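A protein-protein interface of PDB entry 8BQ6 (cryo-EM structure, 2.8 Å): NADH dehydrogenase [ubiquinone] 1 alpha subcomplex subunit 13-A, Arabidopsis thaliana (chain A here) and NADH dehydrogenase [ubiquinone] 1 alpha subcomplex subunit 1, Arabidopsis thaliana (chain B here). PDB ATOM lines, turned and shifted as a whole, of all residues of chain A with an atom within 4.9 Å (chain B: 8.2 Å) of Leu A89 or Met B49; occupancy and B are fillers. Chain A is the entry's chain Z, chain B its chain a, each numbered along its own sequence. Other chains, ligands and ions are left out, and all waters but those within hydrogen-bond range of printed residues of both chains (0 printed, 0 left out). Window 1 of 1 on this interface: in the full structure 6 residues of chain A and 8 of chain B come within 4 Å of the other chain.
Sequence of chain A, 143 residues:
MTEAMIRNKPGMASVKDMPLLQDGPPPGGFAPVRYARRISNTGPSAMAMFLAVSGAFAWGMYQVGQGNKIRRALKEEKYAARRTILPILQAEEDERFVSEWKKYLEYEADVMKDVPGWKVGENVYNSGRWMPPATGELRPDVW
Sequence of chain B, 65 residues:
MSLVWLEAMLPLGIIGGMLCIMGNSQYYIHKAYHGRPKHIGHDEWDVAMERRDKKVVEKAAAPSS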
ATOM      1  N   ILE A  85      18.122  -4.789   1.146  1.00  0.00           N
ATOM      2  CA  ILE A  85      19.562  -4.705   1.353  1.00  0.00           C
ATOM      3  C   ILE A  85      20.322  -4.561   0.052  1.00  0.00           C
ATOM      4  O   ILE A  85      21.559  -4.515   0.065  1.00  0.00           O
ATOM      5  CB  ILE A  85      20.094  -5.924   2.127  1.00  0.00           C
ATOM      6  CG1 ILE A  85      19.894  -7.195   1.303  1.00  0.00           C
ATOM      7  CG2 ILE A  85      19.414  -6.025   3.468  1.00  0.00           C
ATOM      8  CD1 ILE A  85      20.922  -8.249   1.567  1.00  0.00           C
ATOM      9  N   LEU A  86      19.621  -4.508  -1.074  1.00  0.00           N
ATOM     10  CA  LEU A  86      20.278  -4.315  -2.363  1.00  0.00           C
ATOM     11  C   LEU A  86      21.084  -3.021  -2.430  1.00  0.00           C
ATOM     12  O   LEU A  86      22.255  -3.071  -2.850  1.00  0.00           O
ATOM     13  CB  LEU A  86      19.212  -4.389  -3.464  1.00  0.00           C
ATOM     14  CG  LEU A  86      19.580  -4.329  -4.941  1.00  0.00           C
ATOM     15  CD1 LEU A  86      19.666  -2.903  -5.445  1.00  0.00           C
ATOM     16  CD2 LEU A  86      20.875  -5.019  -5.131  1.00  0.00           C
ATOM     17  N   PRO A  87      20.544  -1.850  -2.055  1.00  0.00           N
ATOM     18  CA  PRO A  87      21.310  -0.605  -2.253  1.00  0.00           C
ATOM     19  C   PRO A  87      22.645  -0.556  -1.532  1.00  0.00           C
ATOM     20  O   PRO A  87      23.616  -0.042  -2.101  1.00  0.00           O
ATOM     21  CB  PRO A  87      20.347   0.470  -1.736  1.00  0.00           C
ATOM     22  CG  PRO A  87      19.012  -0.119  -1.931  1.00  0.00           C
ATOM     23  CD  PRO A  87      19.175  -1.558  -1.593  1.00  0.00           C
ATOM     24  N   ILE A  88      22.738  -1.071  -0.307  1.00  0.00           N
ATOM     25  CA  ILE A  88      24.010  -0.986   0.404  1.00  0.00           C
ATOM     26  C   ILE A  88      25.046  -1.903  -0.236  1.00  0.00           C
ATOM     27  O   ILE A  88      26.223  -1.542  -0.354  1.00  0.00           O
ATOM     28  CB  ILE A  88      23.822  -1.278   1.905  1.00  0.00           C
ATOM     29  CG1 ILE A  88      25.139  -1.051   2.644  1.00  0.00           C
ATOM     30  CG2 ILE A  88      23.306  -2.682   2.139  1.00  0.00           C
ATOM     31  CD1 ILE A  88      25.082  -1.382   4.099  1.00  0.00           C
ATOM     32  N   LEU A  89      24.627  -3.094  -0.672  1.00  0.00           N
ATOM     33  CA  LEU A  89      25.556  -3.987  -1.354  1.00  0.00           C
ATOM     34  C   LEU A  89      26.049  -3.373  -2.655  1.00  0.00           C
ATOM     35  O   LEU A  89      27.244  -3.444  -2.973  1.00  0.00           O
ATOM     36  CB  LEU A  89      24.892  -5.335  -1.620  1.00  0.00           C
ATOM     37  CG  LEU A  89      24.365  -6.064  -0.389  1.00  0.00           C
ATOM     38  CD1 LEU A  89      23.401  -7.141  -0.816  1.00  0.00           C
ATOM     39  CD2 LEU A  89      25.511  -6.649   0.418  1.00  0.00           C
ATOM     40  N   GLN A  90      25.144  -2.752  -3.416  1.00  0.00           N
ATOM     41  CA  GLN A  90      25.560  -2.110  -4.657  1.00  0.00           C
ATOM     42  C   GLN A  90      26.493  -0.936  -4.389  1.00  0.00           C
ATOM     43  O   GLN A  90      27.436  -0.705  -5.149  1.00  0.00           O
ATOM     44  CB  GLN A  90      24.342  -1.653  -5.457  1.00  0.00           C
ATOM     45  CG  GLN A  90      24.647  -1.263  -6.897  1.00  0.00           C
ATOM     46  CD  GLN A  90      25.499  -2.285  -7.627  1.00  0.00           C
ATOM     47  OE1 GLN A  90      25.020  -3.353  -8.000  1.00  0.00           O
ATOM     48  NE2 GLN A  90      26.759  -1.949  -7.857  1.00  0.00           N
ATOM     49  N   ALA A  91      26.244  -0.175  -3.319  1.00  0.00           N
ATOM     50  CA  ALA A  91      27.112   0.958  -3.006  1.00  0.00           C
ATOM     51  C   ALA A  91      28.504   0.494  -2.595  1.00  0.00           C
ATOM     52  O   ALA A  91      29.515   1.090  -2.995  1.00  0.00           O
ATOM     53  CB  ALA A  91      26.483   1.811  -1.906  1.00  0.00           C
ATOM     54  N   GLU A  92      28.574  -0.569  -1.793  1.00  0.00           N
ATOM     55  CA  GLU A  92      29.860  -1.168  -1.452  1.00  0.00           C
ATOM     56  C   GLU A  92      30.603  -1.611  -2.706  1.00  0.00           C
ATOM     57  O   GLU A  92      31.797  -1.322  -2.874  1.00  0.00           O
ATOM     58  CB  GLU A  92      29.631  -2.349  -0.512  1.00  0.00           C
ATOM     59  CG  GLU A  92      30.883  -2.972   0.062  1.00  0.00           C
ATOM     60  CD  GLU A  92      30.566  -4.148   0.964  1.00  0.00           C
ATOM     61  OE1 GLU A  92      30.255  -3.922   2.150  1.00  0.00           O
ATOM     62  OE2 GLU A  92      30.627  -5.301   0.489  1.00  0.00           O
ATOM     63  N   GLU A  93      29.904  -2.305  -3.608  1.00  0.00           N
ATOM     64  CA  GLU A  93      30.547  -2.772  -4.831  1.00  0.00           C
ATOM     65  C   GLU A  93      31.000  -1.604  -5.699  1.00  0.00           C
ATOM     66  O   GLU A  93      32.050  -1.672  -6.345  1.00  0.00           O
ATOM     67  CB  GLU A  93      29.600  -3.694  -5.602  1.00  0.00           C
ATOM     68  CG  GLU A  93      29.989  -3.968  -7.052  1.00  0.00           C
ATOM     69  CD  GLU A  93      31.222  -4.847  -7.204  1.00  0.00           C
ATOM     70  OE1 GLU A  93      31.806  -5.280  -6.188  1.00  0.00           O
ATOM     71  OE2 GLU A  93      31.611  -5.109  -8.360  1.00  0.00           O
ATOM     72  N   ARG B  36      28.412 -25.468   8.383  1.00  0.00           N
ATOM     73  CA  ARG B  36      26.969 -25.299   8.434  1.00  0.00           C
ATOM     74  C   ARG B  36      26.353 -26.251   7.422  1.00  0.00           C
ATOM     75  O   ARG B  36      27.029 -26.688   6.485  1.00  0.00           O
ATOM     76  CB  ARG B  36      26.554 -23.851   8.138  1.00  0.00           C
ATOM     77  CG  ARG B  36      27.227 -23.222   6.947  1.00  0.00           C
ATOM     78  CD  ARG B  36      26.756 -21.790   6.818  1.00  0.00           C
ATOM     79  NE  ARG B  36      27.345 -21.089   5.685  1.00  0.00           N
ATOM     80  CZ  ARG B  36      26.980 -19.877   5.296  1.00  0.00           C
ATOM     81  NH1 ARG B  36      26.013 -19.217   5.914  1.00  0.00           N
ATOM     82  NH2 ARG B  36      27.603 -19.308   4.269  1.00  0.00           N
ATOM     83  N   HIS B  42      20.886 -22.890  -3.609  1.00  0.00           N
ATOM     84  CA  HIS B  42      21.966 -21.919  -3.700  1.00  0.00           C
ATOM     85  C   HIS B  42      21.976 -21.300  -5.087  1.00  0.00           C
ATOM     86  O   HIS B  42      22.303 -21.965  -6.074  1.00  0.00           O
ATOM     87  CB  HIS B  42      23.298 -22.593  -3.399  1.00  0.00           C
ATOM     88  CG  HIS B  42      24.215 -21.751  -2.578  1.00  0.00           C
ATOM     89  ND1 HIS B  42      23.904 -21.347  -1.298  1.00  0.00           N
ATOM     90  CD2 HIS B  42      25.428 -21.219  -2.857  1.00  0.00           C
ATOM     91  CE1 HIS B  42      24.890 -20.612  -0.819  1.00  0.00           C
ATOM     92  NE2 HIS B  42      25.827 -20.517  -1.746  1.00  0.00           N
ATOM     93  N   ASP B  43      21.627 -20.028  -5.167  1.00  0.00           N
ATOM     94  CA  ASP B  43      21.558 -19.340  -6.437  1.00  0.00           C
ATOM     95  C   ASP B  43      22.705 -18.336  -6.565  1.00  0.00           C
ATOM     96  O   ASP B  43      23.619 -18.282  -5.733  1.00  0.00           O
ATOM     97  CB  ASP B  43      20.168 -18.708  -6.610  1.00  0.00           C
ATOM     98  CG  ASP B  43      19.893 -17.588  -5.618  1.00  0.00           C
ATOM     99  OD1 ASP B  43      18.728 -17.444  -5.187  1.00  0.00           O
ATOM    100  OD2 ASP B  43      20.824 -16.853  -5.260  1.00  0.00           O
ATOM    101  N   GLU B  44      22.647 -17.549  -7.638  1.00  0.00           N
ATOM    102  CA  GLU B  44      23.677 -16.562  -7.933  1.00  0.00           C
ATOM    103  C   GLU B  44      23.794 -15.537  -6.812  1.00  0.00           C
ATOM    104  O   GLU B  44      24.898 -15.079  -6.490  1.00  0.00           O
ATOM    105  CB  GLU B  44      23.358 -15.859  -9.255  1.00  0.00           C
ATOM    106  CG  GLU B  44      22.960 -16.741 -10.462  1.00  0.00           C
ATOM    107  CD  GLU B  44      21.778 -17.677 -10.217  1.00  0.00           C
ATOM    108  OE1 GLU B  44      20.675 -17.195  -9.928  1.00  0.00           O
ATOM    109  OE2 GLU B  44      21.954 -18.904 -10.325  1.00  0.00           O
ATOM    110  N   TRP B  45      22.662 -15.153  -6.221  1.00  0.00           N
ATOM    111  CA  TRP B  45      22.692 -14.209  -5.110  1.00  0.00           C
ATOM    112  C   TRP B  45      23.468 -14.777  -3.932  1.00  0.00           C
ATOM    113  O   TRP B  45      24.323 -14.100  -3.361  1.00  0.00           O
ATOM    114  CB  TRP B  45      21.268 -13.849  -4.688  1.00  0.00           C
ATOM    115  CG  TRP B  45      21.200 -12.894  -3.541  1.00  0.00           C
ATOM    116  CD1 TRP B  45      21.230 -13.207  -2.217  1.00  0.00           C
ATOM    117  CD2 TRP B  45      21.063 -11.470  -3.613  1.00  0.00           C
ATOM    118  NE1 TRP B  45      21.133 -12.071  -1.458  1.00  0.00           N
ATOM    119  CE2 TRP B  45      21.027 -10.989  -2.292  1.00  0.00           C
ATOM    120  CE3 TRP B  45      20.969 -10.557  -4.665  1.00  0.00           C
ATOM    121  CZ2 TRP B  45      20.903  -9.637  -1.993  1.00  0.00           C
ATOM    122  CZ3 TRP B  45      20.845  -9.216  -4.367  1.00  0.00           C
ATOM    123  CH2 TRP B  45      20.815  -8.768  -3.042  1.00  0.00           C
ATOM    124  N   ASP B  46      23.171 -16.020  -3.547  1.00  0.00           N
ATOM    125  CA  ASP B  46      23.850 -16.627  -2.405  1.00  0.00           C
ATOM    126  C   ASP B  46      25.335 -16.801  -2.675  1.00  0.00           C
ATOM    127  O   ASP B  46      26.165 -16.625  -1.773  1.00  0.00           O
ATOM    128  CB  ASP B  46      23.210 -17.970  -2.076  1.00  0.00           C
ATOM    129  CG  ASP B  46      21.752 -17.840  -1.749  1.00  0.00           C
ATOM    130  OD1 ASP B  46      20.932 -18.533  -2.383  1.00  0.00           O
ATOM    131  OD2 ASP B  46      21.423 -17.034  -0.859  1.00  0.00           O
ATOM    132  N   VAL B  47      25.687 -17.158  -3.909  1.00  0.00           N
ATOM    133  CA  VAL B  47      27.093 -17.262  -4.280  1.00  0.00           C
ATOM    134  C   VAL B  47      27.778 -15.908  -4.141  1.00  0.00           C
ATOM    135  O   VAL B  47      28.872 -15.802  -3.567  1.00  0.00           O
ATOM    136  CB  VAL B  47      27.214 -17.829  -5.707  1.00  0.00           C
ATOM    137  CG1 VAL B  47      28.639 -17.754  -6.189  1.00  0.00           C
ATOM    138  CG2 VAL B  47      26.724 -19.267  -5.742  1.00  0.00           C
ATOM    139  N   ALA B  48      27.137 -14.849  -4.640  1.00  0.00           N
ATOM    140  CA  ALA B  48      27.718 -13.513  -4.544  1.00  0.00           C
ATOM    141  C   ALA B  48      27.808 -13.048  -3.094  1.00  0.00           C
ATOM    142  O   ALA B  48      28.751 -12.346  -2.717  1.00  0.00           O
ATOM    143  CB  ALA B  48      26.900 -12.529  -5.378  1.00  0.00           C
ATOM    144  N   MET B  49      26.829 -13.428  -2.269  1.00  0.00           N
ATOM    145  CA  MET B  49      26.866 -13.088  -0.851  1.00  0.00           C
ATOM    146  C   MET B  49      28.025 -13.778  -0.157  1.00  0.00           C
ATOM    147  O   MET B  49      28.681 -13.194   0.705  1.00  0.00           O
ATOM    148  CB  MET B  49      25.553 -13.466  -0.167  1.00  0.00           C
ATOM    149  CG  MET B  49      24.341 -12.676  -0.605  1.00  0.00           C
ATOM    150  SD  MET B  49      24.333 -10.974  -0.029  1.00  0.00           S
ATOM    151  CE  MET B  49      25.106 -10.168  -1.427  1.00  0.00           C
ATOM    152  N   GLU B  50      28.273 -15.041  -0.500  1.00  0.00           N
ATOM    153  CA  GLU B  50      29.406 -15.741   0.089  1.00  0.00           C
ATOM    154  C   GLU B  50      30.727 -15.110  -0.340  1.00  0.00           C
ATOM    155  O   GLU B  50      31.633 -14.916   0.484  1.00  0.00           O
ATOM    156  CB  GLU B  50      29.351 -17.217  -0.292  1.00  0.00           C
ATOM    157  CG  GLU B  50      30.599 -17.985   0.058  1.00  0.00           C
ATOM    158  CD  GLU B  50      30.487 -19.453  -0.285  1.00  0.00           C
ATOM    159  OE1 GLU B  50      31.519 -20.153  -0.233  1.00  0.00           O
ATOM    160  OE2 GLU B  50      29.367 -19.907  -0.605  1.00  0.00           O
ATOM    161  N   ARG B  51      30.845 -14.757  -1.624  1.00  0.00           N
ATOM    162  CA  ARG B  51      32.085 -14.154  -2.110  1.00  0.00           C
ATOM    163  C   ARG B  51      32.323 -12.783  -1.490  1.00  0.00           C
ATOM    164  O   ARG B  51      33.470 -12.398  -1.240  1.00  0.00           O
ATOM    165  CB  ARG B  51      32.063 -14.051  -3.633  1.00  0.00           C
ATOM    166  CG  ARG B  51      32.475 -15.327  -4.325  1.00  0.00           C
ATOM    167  CD  ARG B  51      31.831 -15.444  -5.684  1.00  0.00           C
ATOM    168  NE  ARG B  51      31.885 -16.817  -6.168  1.00  0.00           N
ATOM    169  CZ  ARG B  51      31.904 -17.158  -7.447  1.00  0.00           C
ATOM    170  NH1 ARG B  51      31.881 -16.246  -8.405  1.00  0.00           N
ATOM    171  NH2 ARG B  51      31.945 -18.446  -7.774  1.00  0.00           N
ATOM    172  N   ARG B  52      31.256 -12.020  -1.257  1.00  0.00           N
ATOM    173  CA  ARG B  52      31.406 -10.727  -0.602  1.00  0.00           C
ATOM    174  C   ARG B  52      31.680 -10.881   0.890  1.00  0.00           C
ATOM    175  O   ARG B  52      32.488 -10.131   1.457  1.00  0.00           O
ATOM    176  CB  ARG B  52      30.150  -9.897  -0.843  1.00  0.00           C
ATOM    177  CG  ARG B  52      30.186  -8.501  -0.288  1.00  0.00           C
ATOM    178  CD  ARG B  52      28.831  -8.168   0.285  1.00  0.00           C
ATOM    179  NE  ARG B  52      28.883  -7.101   1.274  1.00  0.00           N
ATOM    180  CZ  ARG B  52      28.564  -7.254   2.551  1.00  0.00           C
ATOM    181  NH1 ARG B  52      28.231  -8.436   3.044  1.00  0.00           N
ATOM    182  NH2 ARG B  52      28.579  -6.194   3.354  1.00  0.00           N
ATOM    183  N   ASP B  53      31.022 -11.848   1.532  1.00  0.00           N
ATOM    184  CA  ASP B  53      31.219 -12.110   2.949  1.00  0.00           C
ATOM    185  C   ASP B  53      32.639 -12.546   3.245  1.00  0.00           C
ATOM    186  O   ASP B  53      33.150 -12.270   4.334  1.00  0.00           O
ATOM    187  CB  ASP B  53      30.248 -13.189   3.417  1.00  0.00           C
ATOM    188  CG  ASP B  53      29.007 -12.620   4.045  1.00  0.00           C
ATOM    189  OD1 ASP B  53      28.679 -11.449   3.770  1.00  0.00           O
ATOM    190  OD2 ASP B  53      28.352 -13.352   4.811  1.00  0.00           O
ATOM    191  N   LYS B  54      33.285 -13.236   2.305  1.00  0.00           N
ATOM    192  CA  LYS B  54      34.692 -13.567   2.503  1.00  0.00           C
ATOM    193  C   LYS B  54      35.514 -12.308   2.742  1.00  0.00           C
ATOM    194  O   LYS B  54      36.315 -12.246   3.680  1.00  0.00           O
ATOM    195  CB  LYS B  54      35.235 -14.342   1.304  1.00  0.00           C
ATOM    196  CG  LYS B  54      34.627 -15.720   1.129  1.00  0.00           C
ATOM    197  CD  LYS B  54      35.598 -16.659   0.436  1.00  0.00           C
ATOM    198  CE  LYS B  54      34.882 -17.596  -0.521  1.00  0.00           C
ATOM    199  NZ  LYS B  54      35.676 -17.851  -1.757  1.00  0.00           N
ATOM    200  N   LYS B  55      35.315 -11.285   1.910  1.00  0.00           N
ATOM    201  CA  LYS B  55      36.052 -10.038   2.084  1.00  0.00           C
ATOM    202  C   LYS B  55      35.638  -9.326   3.363  1.00  0.00           C
ATOM    203  O   LYS B  55      36.486  -8.913   4.162  1.00  0.00           O
ATOM    204  CB  LYS B  55      35.835  -9.128   0.879  1.00  0.00           C
ATOM    205  CG  LYS B  55      36.439  -9.658  -0.393  1.00  0.00           C
ATOM    206  CD  LYS B  55      36.165  -8.723  -1.544  1.00  0.00           C
ATOM    207  CE  LYS B  55      36.804  -9.262  -2.809  1.00  0.00           C
ATOM    208  NZ  LYS B  55      36.550  -8.397  -3.991  1.00  0.00           N
ATOM    209  N   VAL B  56      34.328  -9.183   3.581  1.00  0.00           N
ATOM    210  CA  VAL B  56      33.833  -8.479   4.761  1.00  0.00           C
ATOM    211  C   VAL B  56      34.276  -9.147   6.064  1.00  0.00           C
ATOM    212  O   VAL B  56      34.389  -8.473   7.094  1.00  0.00           O
ATOM    213  CB  VAL B  56      32.297  -8.344   4.668  1.00  0.00           C
ATOM    214  CG1 VAL B  56      31.759  -7.449   5.763  1.00  0.00           C
ATOM    215  CG2 VAL B  56      31.918  -7.761   3.322  1.00  0.00           C
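The side-chain carboxylate of Glu A92 is in salt-bridge range of the guanidinium group of Arg B52, 2.6 Å away.
The side-chain carboxylate (OD2) of Asp B43 lies within hydrogen-bond range of the backbone NH (N) of Trp B45 (2.7 Å).
The indole nitrogen of Trp B45 sits close to the side-chain sulfur of Met B49, 3.7 Å away.
The side-chain carboxylate of Asp B53 is in salt-bridge range of the guanidinium group of Arg B52, at 3.1 Å.
Trp B45 touches Ile A85 (CZ2 to CD1, 3.8 Å).
CZ2 of Trp B45 touches CD1 of Leu A89, at 3.7 Å.
Met B49 touches Leu A89.
Leu A89 touches Arg B52.
Glu A92 touches Val B56.
Pro A87 touches none of the printed residues of chain B.
Of chain B, only Trp B45 (3.7 Å), Met B49 (3.5 Å) and Arg B52 (3.5 Å) come within 4 Å of Leu A89.
Of the printed residues of chain B, Glu A92 touches Arg B52 (2.6 Å) and Val B56 (3.97 Å).
Printed residues of chain A within 4 Å of Trp B45: Ile A85 and Leu A89.
Ala B48 touches none of the printed residues of chain A.
Of the printed residues of chain A, Met B49 touches Leu A89.
Of the printed residues of chain A, Arg B52 touches Leu A89 and Glu A92.
Of the printed residues of chain A, Val B56 touches Glu A92 (3.97 Å).
The nearest residue of chain A that does not touch Met B49 is Ile A85 (4.6 Å).
Hydrophobic or aromatic side chains of chain B that line the printed part of chain A: Trp B45, Met B49 and Val B56.
Of the 9 printed residues of chain A, 3 touch a printed residue of chain B.
Printed residues of chain A that touch a printed residue of chain B: Ile A85, Leu A89 and Glu A92.
Hydrophobic or aromatic side chains of chain A within 4 Å of the printed part of chain B: Ile A85 and Leu A89.
Among the printed residues, Asp or Glu carboxylates within 4 Å of a Lys or Arg side-chain nitrogen of the other chain: Glu A92 with Arg B52 (2.6 Å).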
